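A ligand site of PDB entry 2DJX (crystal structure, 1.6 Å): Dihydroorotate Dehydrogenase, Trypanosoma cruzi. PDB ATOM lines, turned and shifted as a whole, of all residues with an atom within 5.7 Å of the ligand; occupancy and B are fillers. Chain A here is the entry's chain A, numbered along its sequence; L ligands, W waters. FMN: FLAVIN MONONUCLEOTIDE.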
ATOM      1  N   ALA A  20     -12.235  12.694  -4.374  1.00  0.00           N
ATOM      2  CA  ALA A  20     -13.322  11.946  -3.734  1.00  0.00           C
ATOM      3  C   ALA A  20     -14.579  12.055  -4.618  1.00  0.00           C
ATOM      4  O   ALA A  20     -14.824  13.108  -5.238  1.00  0.00           O
ATOM      5  CB  ALA A  20     -13.600  12.496  -2.319  1.00  0.00           C
ATOM      6  N   ALA A  21     -15.347  10.972  -4.733  1.00  0.00           N
ATOM      7  CA  ALA A  21     -16.583  11.004  -5.553  1.00  0.00           C
ATOM      8  C   ALA A  21     -17.485  12.174  -5.173  1.00  0.00           C
ATOM      9  O   ALA A  21     -17.666  12.463  -3.997  1.00  0.00           O
ATOM     10  CB  ALA A  21     -17.335   9.670  -5.463  1.00  0.00           C
ATOM     11  N   GLY A  22     -18.023  12.853  -6.171  1.00  0.00           N
ATOM     12  CA  GLY A  22     -18.875  14.040  -5.945  1.00  0.00           C
ATOM     13  C   GLY A  22     -18.220  15.406  -6.051  1.00  0.00           C
ATOM     14  O   GLY A  22     -18.910  16.413  -6.274  1.00  0.00           O
ATOM     15  N   VAL A  23     -16.890  15.457  -5.880  1.00  0.00           N
ATOM     16  CA  VAL A  23     -16.150  16.737  -5.949  1.00  0.00           C
ATOM     17  C   VAL A  23     -15.446  16.865  -7.315  1.00  0.00           C
ATOM     18  O   VAL A  23     -14.691  15.974  -7.727  1.00  0.00           O
ATOM     19  CB  VAL A  23     -15.142  16.886  -4.767  1.00  0.00           C
ATOM     20  CG1 VAL A  23     -14.302  18.170  -4.911  1.00  0.00           C
ATOM     21  CG2 VAL A  23     -15.873  16.865  -3.429  1.00  0.00           C
ATOM     22  N   LYS A  45     -19.037  11.559 -10.537  1.00  0.00           N
ATOM     23  CA  LYS A  45     -20.131  11.783  -9.570  1.00  0.00           C
ATOM     24  C   LYS A  45     -21.052  10.544  -9.436  1.00  0.00           C
ATOM     25  O   LYS A  45     -21.427   9.949 -10.445  1.00  0.00           O
ATOM     26  CB  LYS A  45     -20.969  12.999 -10.030  1.00  0.00           C
ATOM     27  CG  LYS A  45     -22.306  13.192  -9.282  1.00  0.00           C
ATOM     28  CD  LYS A  45     -22.083  13.677  -7.832  1.00  0.00           C
ATOM     29  CE  LYS A  45     -23.332  13.522  -6.976  1.00  0.00           C
ATOM     30  NZ  LYS A  45     -23.033  13.990  -5.566  1.00  0.00           N
ATOM     31  N   SER A  46     -21.447  10.174  -8.209  1.00  0.00           N
ATOM     32  CA  SER A  46     -22.374   9.025  -8.032  1.00  0.00           C
ATOM     33  C   SER A  46     -23.643   9.266  -8.860  1.00  0.00           C
ATOM     34  O   SER A  46     -24.256  10.332  -8.734  1.00  0.00           O
ATOM     35  CB  SER A  46     -22.758   8.789  -6.558  1.00  0.00           C
ATOM     36  OG  SER A  46     -21.669   8.260  -5.814  1.00  0.00           O
ATOM     37  N   TYR A  60     -24.515  23.279   0.300  1.00  0.00           N
ATOM     38  CA  TYR A  60     -23.119  23.067   0.714  1.00  0.00           C
ATOM     39  C   TYR A  60     -22.580  24.339   1.403  1.00  0.00           C
ATOM     40  O   TYR A  60     -22.776  25.440   0.883  1.00  0.00           O
ATOM     41  CB  TYR A  60     -22.234  22.703  -0.493  1.00  0.00           C
ATOM     42  CG  TYR A  60     -20.734  22.678  -0.203  1.00  0.00           C
ATOM     43  CD1 TYR A  60     -19.940  23.836  -0.384  1.00  0.00           C
ATOM     44  CD2 TYR A  60     -20.098  21.509   0.244  1.00  0.00           C
ATOM     45  CE1 TYR A  60     -18.562  23.824  -0.105  1.00  0.00           C
ATOM     46  CE2 TYR A  60     -18.719  21.485   0.517  1.00  0.00           C
ATOM     47  CZ  TYR A  60     -17.954  22.639   0.328  1.00  0.00           C
ATOM     48  OH  TYR A  60     -16.599  22.595   0.620  1.00  0.00           O
ATOM     49  N   SER A  67     -16.508  20.942   6.138  1.00  0.00           N
ATOM     50  CA  SER A  67     -17.737  21.251   5.375  1.00  0.00           C
ATOM     51  C   SER A  67     -18.964  20.460   5.863  1.00  0.00           C
ATOM     52  O   SER A  67     -18.829  19.412   6.502  1.00  0.00           O
ATOM     53  CB  SER A  67     -17.518  21.003   3.874  1.00  0.00           C
ATOM     54  OG  SER A  67     -17.365  19.619   3.586  1.00  0.00           O
ATOM     55  N   ASN A  69     -22.826  19.212   3.984  1.00  0.00           N
ATOM     56  CA  ASN A  69     -23.606  19.172   2.731  1.00  0.00           C
ATOM     57  C   ASN A  69     -24.822  18.271   2.801  1.00  0.00           C
ATOM     58  O   ASN A  69     -24.828  17.274   3.535  1.00  0.00           O
ATOM     59  CB  ASN A  69     -22.704  18.783   1.553  1.00  0.00           C
ATOM     60  CG  ASN A  69     -22.679  17.269   1.289  1.00  0.00           C
ATOM     61  OD1 ASN A  69     -23.627  16.682   0.710  1.00  0.00           O
ATOM     62  ND2 ASN A  69     -21.604  16.623   1.686  1.00  0.00           N
ATOM     63  N   MET A  71     -26.414  17.359  -0.626  1.00  0.00           N
ATOM     64  CA  MET A  71     -26.573  17.604  -2.080  1.00  0.00           C
ATOM     65  C   MET A  71     -27.815  16.934  -2.675  1.00  0.00           C
ATOM     66  O   MET A  71     -28.509  17.549  -3.507  1.00  0.00           O
ATOM     67  CB  MET A  71     -25.335  17.176  -2.888  1.00  0.00           C
ATOM     68  CG  MET A  71     -23.962  17.719  -2.467  1.00  0.00           C
ATOM     69  SD  MET A  71     -23.842  19.514  -2.347  1.00  0.00           S
ATOM     70  CE  MET A  71     -23.807  19.958  -4.085  1.00  0.00           C
ATOM     71  N   LEU A  73     -27.806  13.761  -4.322  1.00  0.00           N
ATOM     72  CA  LEU A  73     -27.425  13.070  -5.564  1.00  0.00           C
ATOM     73  C   LEU A  73     -27.780  13.798  -6.896  1.00  0.00           C
ATOM     74  O   LEU A  73     -28.313  13.192  -7.831  1.00  0.00           O
ATOM     75  CB  LEU A  73     -27.956  11.604  -5.581  1.00  0.00           C
ATOM     76  CG  LEU A  73     -27.362  10.577  -4.605  1.00  0.00           C
ATOM     77  CD1 LEU A  73     -28.186   9.273  -4.637  1.00  0.00           C
ATOM     78  CD2 LEU A  73     -25.872  10.288  -4.874  1.00  0.00           C
ATOM     79  N   SER A  99     -18.673   5.885 -10.318  1.00  0.00           N
ATOM     80  CA  SER A  99     -19.455   5.620  -9.095  1.00  0.00           C
ATOM     81  C   SER A  99     -20.948   5.542  -9.406  1.00  0.00           C
ATOM     82  O   SER A  99     -21.476   6.393 -10.120  1.00  0.00           O
ATOM     83  CB  SER A  99     -19.198   6.706  -8.046  1.00  0.00           C
ATOM     84  OG  SER A  99     -20.024   6.510  -6.888  1.00  0.00           O
ATOM     85  N   GLU A 127     -17.032   1.799  -8.630  1.00  0.00           N
ATOM     86  CA  GLU A 127     -17.169   2.050  -7.177  1.00  0.00           C
ATOM     87  C   GLU A 127     -18.669   2.110  -6.808  1.00  0.00           C
ATOM     88  O   GLU A 127     -19.384   3.027  -7.202  1.00  0.00           O
ATOM     89  CB  GLU A 127     -16.437   3.350  -6.744  1.00  0.00           C
ATOM     90  CG  GLU A 127     -16.421   3.588  -5.193  1.00  0.00           C
ATOM     91  CD  GLU A 127     -15.586   4.789  -4.758  1.00  0.00           C
ATOM     92  OE1 GLU A 127     -16.140   5.899  -4.665  1.00  0.00           O
ATOM     93  OE2 GLU A 127     -14.371   4.623  -4.469  1.00  0.00           O
ATOM     94  N   ASN A 129     -21.638   2.786  -4.351  1.00  0.00           N
ATOM     95  CA  ASN A 129     -21.901   3.639  -3.176  1.00  0.00           C
ATOM     96  C   ASN A 129     -22.994   3.075  -2.259  1.00  0.00           C
ATOM     97  O   ASN A 129     -24.191   3.118  -2.604  1.00  0.00           O
ATOM     98  CB  ASN A 129     -22.257   5.076  -3.657  1.00  0.00           C
ATOM     99  CG  ASN A 129     -22.437   6.092  -2.507  1.00  0.00           C
ATOM    100  OD1 ASN A 129     -22.381   5.767  -1.325  1.00  0.00           O
ATOM    101  ND2 ASN A 129     -22.647   7.360  -2.893  1.00  0.00           N
ATOM    102  N   SER A 131     -23.446   4.228   1.005  1.00  0.00           N
ATOM    103  CA  SER A 131     -23.310   5.102   2.178  1.00  0.00           C
ATOM    104  C   SER A 131     -23.802   6.555   2.018  1.00  0.00           C
ATOM    105  O   SER A 131     -23.460   7.425   2.835  1.00  0.00           O
ATOM    106  CB  SER A 131     -21.857   5.069   2.664  1.00  0.00           C
ATOM    107  OG  SER A 131     -20.942   5.223   1.579  1.00  0.00           O
ATOM    108  N   LYS A 166     -17.876   1.857  -1.580  1.00  0.00           N
ATOM    109  CA  LYS A 166     -17.734   3.067  -0.732  1.00  0.00           C
ATOM    110  C   LYS A 166     -18.552   2.912   0.567  1.00  0.00           C
ATOM    111  O   LYS A 166     -19.799   2.811   0.525  1.00  0.00           O
ATOM    112  CB  LYS A 166     -18.165   4.329  -1.506  1.00  0.00           C
ATOM    113  CG  LYS A 166     -18.037   5.674  -0.722  1.00  0.00           C
ATOM    114  CD  LYS A 166     -16.590   6.185  -0.681  1.00  0.00           C
ATOM    115  CE  LYS A 166     -16.465   7.661  -0.194  1.00  0.00           C
ATOM    116  NZ  LYS A 166     -16.832   8.674  -1.228  1.00  0.00           N
ATOM    117  N   VAL A 195     -13.561   6.760   4.110  1.00  0.00           N
ATOM    118  CA  VAL A 195     -15.001   6.718   4.387  1.00  0.00           C
ATOM    119  C   VAL A 195     -15.790   7.783   3.582  1.00  0.00           C
ATOM    120  O   VAL A 195     -15.198   8.783   3.119  1.00  0.00           O
ATOM    121  CB  VAL A 195     -15.295   7.019   5.893  1.00  0.00           C
ATOM    122  CG1 VAL A 195     -14.740   5.948   6.777  1.00  0.00           C
ATOM    123  CG2 VAL A 195     -14.725   8.398   6.329  1.00  0.00           C
ATOM    124  N   ASN A 196     -17.105   7.561   3.438  1.00  0.00           N
ATOM    125  CA  ASN A 196     -18.080   8.615   3.087  1.00  0.00           C
ATOM    126  C   ASN A 196     -18.227   9.605   4.266  1.00  0.00           C
ATOM    127  O   ASN A 196     -17.623   9.394   5.344  1.00  0.00           O
ATOM    128  CB  ASN A 196     -19.455   7.985   2.715  1.00  0.00           C
ATOM    129  CG  ASN A 196     -20.204   8.781   1.642  1.00  0.00           C
ATOM    130  OD1 ASN A 196     -20.247  10.019   1.678  1.00  0.00           O
ATOM    131  ND2 ASN A 196     -20.795   8.069   0.676  1.00  0.00           N
ATOM    132  N   SER A 197     -19.015  10.670   4.069  1.00  0.00           N
ATOM    133  CA  SER A 197     -19.221  11.731   5.098  1.00  0.00           C
ATOM    134  C   SER A 197     -19.747  11.181   6.419  1.00  0.00           C
ATOM    135  O   SER A 197     -20.478  10.166   6.439  1.00  0.00           O
ATOM    136  CB  SER A 197     -20.238  12.769   4.590  1.00  0.00           C
ATOM    137  OG  SER A 197     -19.937  13.259   3.284  1.00  0.00           O
ATOM    138  N   LEU A 222     -20.757  15.548   7.205  1.00  0.00           N
ATOM    139  CA  LEU A 222     -19.548  16.285   7.572  1.00  0.00           C
ATOM    140  C   LEU A 222     -18.298  15.733   6.892  1.00  0.00           C
ATOM    141  O   LEU A 222     -18.075  14.515   6.840  1.00  0.00           O
ATOM    142  CB  LEU A 222     -19.325  16.264   9.092  1.00  0.00           C
ATOM    143  CG  LEU A 222     -20.467  16.757   9.988  1.00  0.00           C
ATOM    144  CD1 LEU A 222     -20.153  16.449  11.468  1.00  0.00           C
ATOM    145  CD2 LEU A 222     -20.768  18.246   9.812  1.00  0.00           C
ATOM    146  N   GLY A 223     -17.457  16.654   6.429  1.00  0.00           N
ATOM    147  CA  GLY A 223     -16.116  16.367   5.886  1.00  0.00           C
ATOM    148  C   GLY A 223     -15.059  17.358   6.377  1.00  0.00           C
ATOM    149  O   GLY A 223     -15.375  18.371   7.021  1.00  0.00           O
ATOM    150  N   GLY A 224     -13.794  17.058   6.080  1.00  0.00           N
ATOM    151  CA  GLY A 224     -12.681  17.963   6.424  1.00  0.00           C
ATOM    152  C   GLY A 224     -11.946  17.665   7.725  1.00  0.00           C
ATOM    153  O   GLY A 224     -11.876  16.508   8.184  1.00  0.00           O
ATOM    154  N   ILE A 227     -13.065  15.215  10.681  1.00  0.00           N
ATOM    155  CA  ILE A 227     -13.263  13.759  10.525  1.00  0.00           C
ATOM    156  C   ILE A 227     -11.977  12.912  10.368  1.00  0.00           C
ATOM    157  O   ILE A 227     -12.075  11.693  10.187  1.00  0.00           O
ATOM    158  CB  ILE A 227     -14.320  13.386   9.391  1.00  0.00           C
ATOM    159  CG1 ILE A 227     -13.753  13.515   7.964  1.00  0.00           C
ATOM    160  CG2 ILE A 227     -15.623  14.221   9.540  1.00  0.00           C
ATOM    161  CD1 ILE A 227     -14.584  12.756   6.878  1.00  0.00           C
ATOM    162  N   CYS A 250     -10.139   7.907   2.489  1.00  0.00           N
ATOM    163  CA  CYS A 250     -10.848   9.163   2.174  1.00  0.00           C
ATOM    164  C   CYS A 250     -11.301   9.793   3.492  1.00  0.00           C
ATOM    165  O   CYS A 250     -11.885   9.110   4.337  1.00  0.00           O
ATOM    166  CB  CYS A 250     -12.072   8.893   1.269  1.00  0.00           C
ATOM    167  SG  CYS A 250     -12.861  10.423   0.606  1.00  0.00           S
ATOM    168  N   GLY A 251     -10.979  11.072   3.687  1.00  0.00           N
ATOM    169  CA  GLY A 251     -11.473  11.833   4.835  1.00  0.00           C
ATOM    170  C   GLY A 251     -10.400  12.660   5.538  1.00  0.00           C
ATOM    171  O   GLY A 251      -9.431  12.125   6.067  1.00  0.00           O
ATOM    172  N   GLY A 252     -10.568  13.976   5.507  1.00  0.00           N
ATOM    173  CA  GLY A 252      -9.668  14.890   6.228  1.00  0.00           C
ATOM    174  C   GLY A 252      -8.275  15.109   5.645  1.00  0.00           C
ATOM    175  O   GLY A 252      -7.385  15.574   6.364  1.00  0.00           O
ATOM    176  N   VAL A 253      -8.068  14.816   4.348  1.00  0.00           N
ATOM    177  CA  VAL A 253      -6.749  15.051   3.721  1.00  0.00           C
ATOM    178  C   VAL A 253      -6.595  16.504   3.204  1.00  0.00           C
ATOM    179  O   VAL A 253      -7.323  16.924   2.300  1.00  0.00           O
ATOM    180  CB  VAL A 253      -6.476  14.055   2.552  1.00  0.00           C
ATOM    181  CG1 VAL A 253      -5.096  14.348   1.842  1.00  0.00           C
ATOM    182  CG2 VAL A 253      -6.548  12.605   3.064  1.00  0.00           C
ATOM    183  N   GLN A 271      -7.976   9.617  -1.430  1.00  0.00           N
ATOM    184  CA  GLN A 271      -8.967  10.504  -2.086  1.00  0.00           C
ATOM    185  C   GLN A 271      -9.093  11.834  -1.324  1.00  0.00           C
ATOM    186  O   GLN A 271      -8.943  11.859  -0.095  1.00  0.00           O
ATOM    187  CB  GLN A 271     -10.345   9.821  -2.169  1.00  0.00           C
ATOM    188  CG  GLN A 271     -10.319   8.372  -2.701  1.00  0.00           C
ATOM    189  CD  GLN A 271     -11.719   7.808  -2.975  1.00  0.00           C
ATOM    190  OE1 GLN A 271     -12.692   8.223  -2.350  1.00  0.00           O
ATOM    191  NE2 GLN A 271     -11.815   6.864  -3.927  1.00  0.00           N
ATOM    192  N   VAL A 272      -9.399  12.920  -2.059  1.00  0.00           N
ATOM    193  CA  VAL A 272      -9.420  14.303  -1.527  1.00  0.00           C
ATOM    194  C   VAL A 272     -10.762  14.980  -1.881  1.00  0.00           C
ATOM    195  O   VAL A 272     -11.085  15.164  -3.079  1.00  0.00           O
ATOM    196  CB  VAL A 272      -8.248  15.136  -2.115  1.00  0.00           C
ATOM    197  CG1 VAL A 272      -8.157  16.510  -1.452  1.00  0.00           C
ATOM    198  CG2 VAL A 272      -6.901  14.349  -1.965  1.00  0.00           C
ATOM    199  N   GLY A 273     -11.539  15.343  -0.842  1.00  0.00           N
ATOM    200  CA  GLY A 273     -12.869  15.934  -1.033  1.00  0.00           C
ATOM    201  C   GLY A 273     -12.930  17.412  -0.707  1.00  0.00           C
ATOM    202  O   GLY A 273     -12.645  18.260  -1.561  1.00  0.00           O
ATOM    203  N   THR A 274     -13.286  17.726   0.550  1.00  0.00           N
ATOM    204  CA  THR A 274     -13.404  19.106   1.030  1.00  0.00           C
ATOM    205  C   THR A 274     -12.225  20.029   0.640  1.00  0.00           C
ATOM    206  O   THR A 274     -12.444  21.146   0.133  1.00  0.00           O
ATOM    207  CB  THR A 274     -13.638  19.130   2.565  1.00  0.00           C
ATOM    208  OG1 THR A 274     -14.888  18.469   2.868  1.00  0.00           O
ATOM    209  CG2 THR A 274     -13.671  20.558   3.133  1.00  0.00           C
ATOM    210  N   ALA A 275     -10.987  19.565   0.865  1.00  0.00           N
ATOM    211  CA  ALA A 275      -9.816  20.393   0.538  1.00  0.00           C
ATOM    212  C   ALA A 275      -9.708  20.730  -0.958  1.00  0.00           C
ATOM    213  O   ALA A 275      -9.320  21.863  -1.313  1.00  0.00           O
ATOM    214  CB  ALA A 275      -8.519  19.745   1.041  1.00  0.00           C
ATOM    215  N   GLN A 277     -12.410  20.821  -3.057  1.00  0.00           N
ATOM    216  CA  GLN A 277     -13.521  21.749  -3.305  1.00  0.00           C
ATOM    217  C   GLN A 277     -13.114  23.211  -2.987  1.00  0.00           C
ATOM    218  O   GLN A 277     -13.490  24.150  -3.725  1.00  0.00           O
ATOM    219  CB  GLN A 277     -14.778  21.316  -2.507  1.00  0.00           C
ATOM    220  CG  GLN A 277     -15.979  22.269  -2.631  1.00  0.00           C
ATOM    221  CD  GLN A 277     -16.533  22.428  -4.068  1.00  0.00           C
ATOM    222  OE1 GLN A 277     -17.051  23.498  -4.427  1.00  0.00           O
ATOM    223  NE2 GLN A 277     -16.426  21.371  -4.880  1.00  0.00           N
HETATM  224  N1  FMN L   1     -19.444  10.566  -1.906  1.00  0.00           N
HETATM  225  C2  FMN L   1     -19.905   9.624  -2.798  1.00  0.00           C
HETATM  226  O2  FMN L   1     -19.602   8.442  -2.643  1.00  0.00           O
HETATM  227  N3  FMN L   1     -20.657  10.016  -3.894  1.00  0.00           N
HETATM  228  C4  FMN L   1     -20.969  11.342  -4.127  1.00  0.00           C
HETATM  229  O4  FMN L   1     -21.567  11.659  -5.176  1.00  0.00           O
HETATM  230  C4A FMN L   1     -20.496  12.312  -3.213  1.00  0.00           C
HETATM  231  N5  FMN L   1     -20.775  13.662  -3.403  1.00  0.00           N
HETATM  232  C5A FMN L   1     -20.249  14.595  -2.523  1.00  0.00           C
HETATM  233  C6  FMN L   1     -20.521  15.953  -2.727  1.00  0.00           C
HETATM  234  C7  FMN L   1     -20.029  16.936  -1.877  1.00  0.00           C
HETATM  235  C7M FMN L   1     -20.038  18.357  -2.384  1.00  0.00           C
HETATM  236  C8  FMN L   1     -19.237  16.551  -0.766  1.00  0.00           C
HETATM  237  C8M FMN L   1     -18.377  17.568  -0.039  1.00  0.00           C
HETATM  238  C9  FMN L   1     -18.977  15.189  -0.555  1.00  0.00           C
HETATM  239  C9A FMN L   1     -19.474  14.211  -1.427  1.00  0.00           C
HETATM  240  N10 FMN L   1     -19.225  12.845  -1.210  1.00  0.00           N
HETATM  241  C10 FMN L   1     -19.727  11.908  -2.110  1.00  0.00           C
HETATM  242  C1' FMN L   1     -18.466  12.396   0.013  1.00  0.00           C
HETATM  243  C2' FMN L   1     -16.966  12.470  -0.320  1.00  0.00           C
HETATM  244  O2' FMN L   1     -16.666  11.588  -1.388  1.00  0.00           O
HETATM  245  C3' FMN L   1     -16.073  12.098   0.872  1.00  0.00           C
HETATM  246  O3' FMN L   1     -16.364  10.760   1.215  1.00  0.00           O
HETATM  247  C4' FMN L   1     -16.267  13.024   2.092  1.00  0.00           C
HETATM  248  O4' FMN L   1     -16.428  14.344   1.630  1.00  0.00           O
HETATM  249  C5' FMN L   1     -15.130  12.935   3.121  1.00  0.00           C
HETATM  250  O5' FMN L   1     -13.864  13.318   2.591  1.00  0.00           O
HETATM  251  P   FMN L   1     -13.231  14.802   2.873  1.00  0.00           P
HETATM  252  O1P FMN L   1     -12.971  14.916   4.359  1.00  0.00           O
HETATM  253  O2P FMN L   1     -11.975  14.917   2.018  1.00  0.00           O
HETATM  254  O3P FMN L   1     -14.273  15.808   2.436  1.00  0.00           O
HETATM  255  O   HOH W   1     -18.313  15.340   3.425  1.00  0.00           O
HETATM  256  O   HOH W   2      -9.789  13.278   2.267  1.00  0.00           O
HETATM  257  O   HOH W   3     -20.009  21.569  -3.721  1.00  0.00           O
HETATM  258  O   HOH W   4     -10.232  17.192   2.304  1.00  0.00           O
HETATM  259  O   HOH W   5     -23.038  10.071  -1.357  1.00  0.00           O
HETATM  260  O   HOH W   6     -18.799   6.242  -4.492  1.00  0.00           O
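The side-chain hydroxyl (OG) of Ser 46 is in hydrogen-bond range of the side-chain hydroxyl (OG) of Ser 99 (2.6 Å). The side-chain hydroxyl of Ser 46 lies within hydrogen-bond range of the side-chain amide nitrogen of Asn 129 (3.2 Å). The side-chain hydroxyl (OG1) of Thr 274 sits at hydrogen-bond distance from the side-chain hydroxyl (OG) of Ser 67 (2.8 Å). N of Ser 131 lies within hydrogen-bond range of OD1 of Asn 129 (3.0 Å). OG of Ser 131 sits at hydrogen-bond distance from O of Lys 166 (2.9 Å). The side-chain hydroxyl (OG) of Ser 131 is in hydrogen-bond range of the side-chain amide nitrogen (ND2) of Asn 196, at 3.0 Å. The backbone carbonyl oxygen (O) of Gly 223 is in hydrogen-bond range of the backbone NH (N) of Ser 67 (2.9 Å). The backbone NH of Val 195 is in hydrogen-bond range of the backbone carbonyl oxygen of Cys 250 (2.9 Å).
Water W1 lies within hydrogen-bond range of OG of Ser 197 (2.6 Å), O4' of the ligand (2.8 Å) and N of Gly 223 (3.4 Å). Water W4 lies within hydrogen-bond range of the backbone NH (N) of Ala 275 (2.9 Å), an oxygen (O2P) of the ligand (2.9 Å) and the backbone carbonyl oxygen (O) of Val 253 (2.9 Å). Water W6 lies within hydrogen-bond range of the side-chain carboxylate (OE1) of Glu 127, the side-chain hydroxyl (OG) of Ser 99 and an oxygen (O2) of the ligand. Water W5 lies within hydrogen-bond range of ND2 of Asn 129 (3.1 Å) and N3 of the ligand (3.5 Å).
O of Val 195 is in hydrogen-bond range of O3' of the ligand. O3P of the ligand lies within hydrogen-bond range of N of Thr 274, at 2.9 Å. The backbone NH (N) of Gly 252 sits at hydrogen-bond distance from an oxygen (O1P) of the ligand (2.8 Å). The backbone carbonyl oxygen of Ala 21 sits close to an oxygen (O2') of the ligand (2.9 Å). O2P of the ligand lies within hydrogen-bond range of N of Gly 273 (2.9 Å). NZ of Lys 45 sits at hydrogen-bond distance from O4 of the ligand (2.8 Å). The side-chain amino group (NZ) of Lys 166 is in hydrogen-bond range of an oxygen (O2') of the ligand (2.9 Å). The side-chain amide nitrogen (ND2) of Asn 129 lies within hydrogen-bond range of an oxygen (O2) of the ligand (3.2 Å). The backbone NH of Gly 224 lies within hydrogen-bond range of an oxygen (O1P) of the ligand. OG1 of Thr 274 lies within hydrogen-bond range of O3P of the ligand (2.8 Å). The side-chain sulfur of Cys 250 lies within hydrogen-bond range of an oxygen (O3') of the ligand, at 3.6 Å. The backbone NH (N) of Ser 46 sits at hydrogen-bond distance from an oxygen (O4) of the ligand, 3.4 Å away. N3 of the ligand sits at hydrogen-bond distance from OG of Ser 46, 2.8 Å away.
CB of Ala 20 touches O2' of the ligand, at 3.3 Å. Gly 22 touches the ligand. Tyr 60 touches the ligand (CE2 to C8M, 3.97 Å). Asn 69 touches the ligand (ND2 to C8, 3.4 Å). Met 71 touches the ligand. Asn 196 touches the ligand. OG of Ser 197 touches C1' of the ligand, at 3.7 Å. Gly 223 touches the ligand. Ile 227 touches the ligand. CA of Gly 251 touches O1P of the ligand, 3.5 Å away. Hydrophobic or aromatic side chains within 4 Å of the ligand: Ala 20, Ala 21, Tyr 60, Met 71 and Ile 227. The nearest printed residue that does not touch the ligand is Val 272 (4.1 Å).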
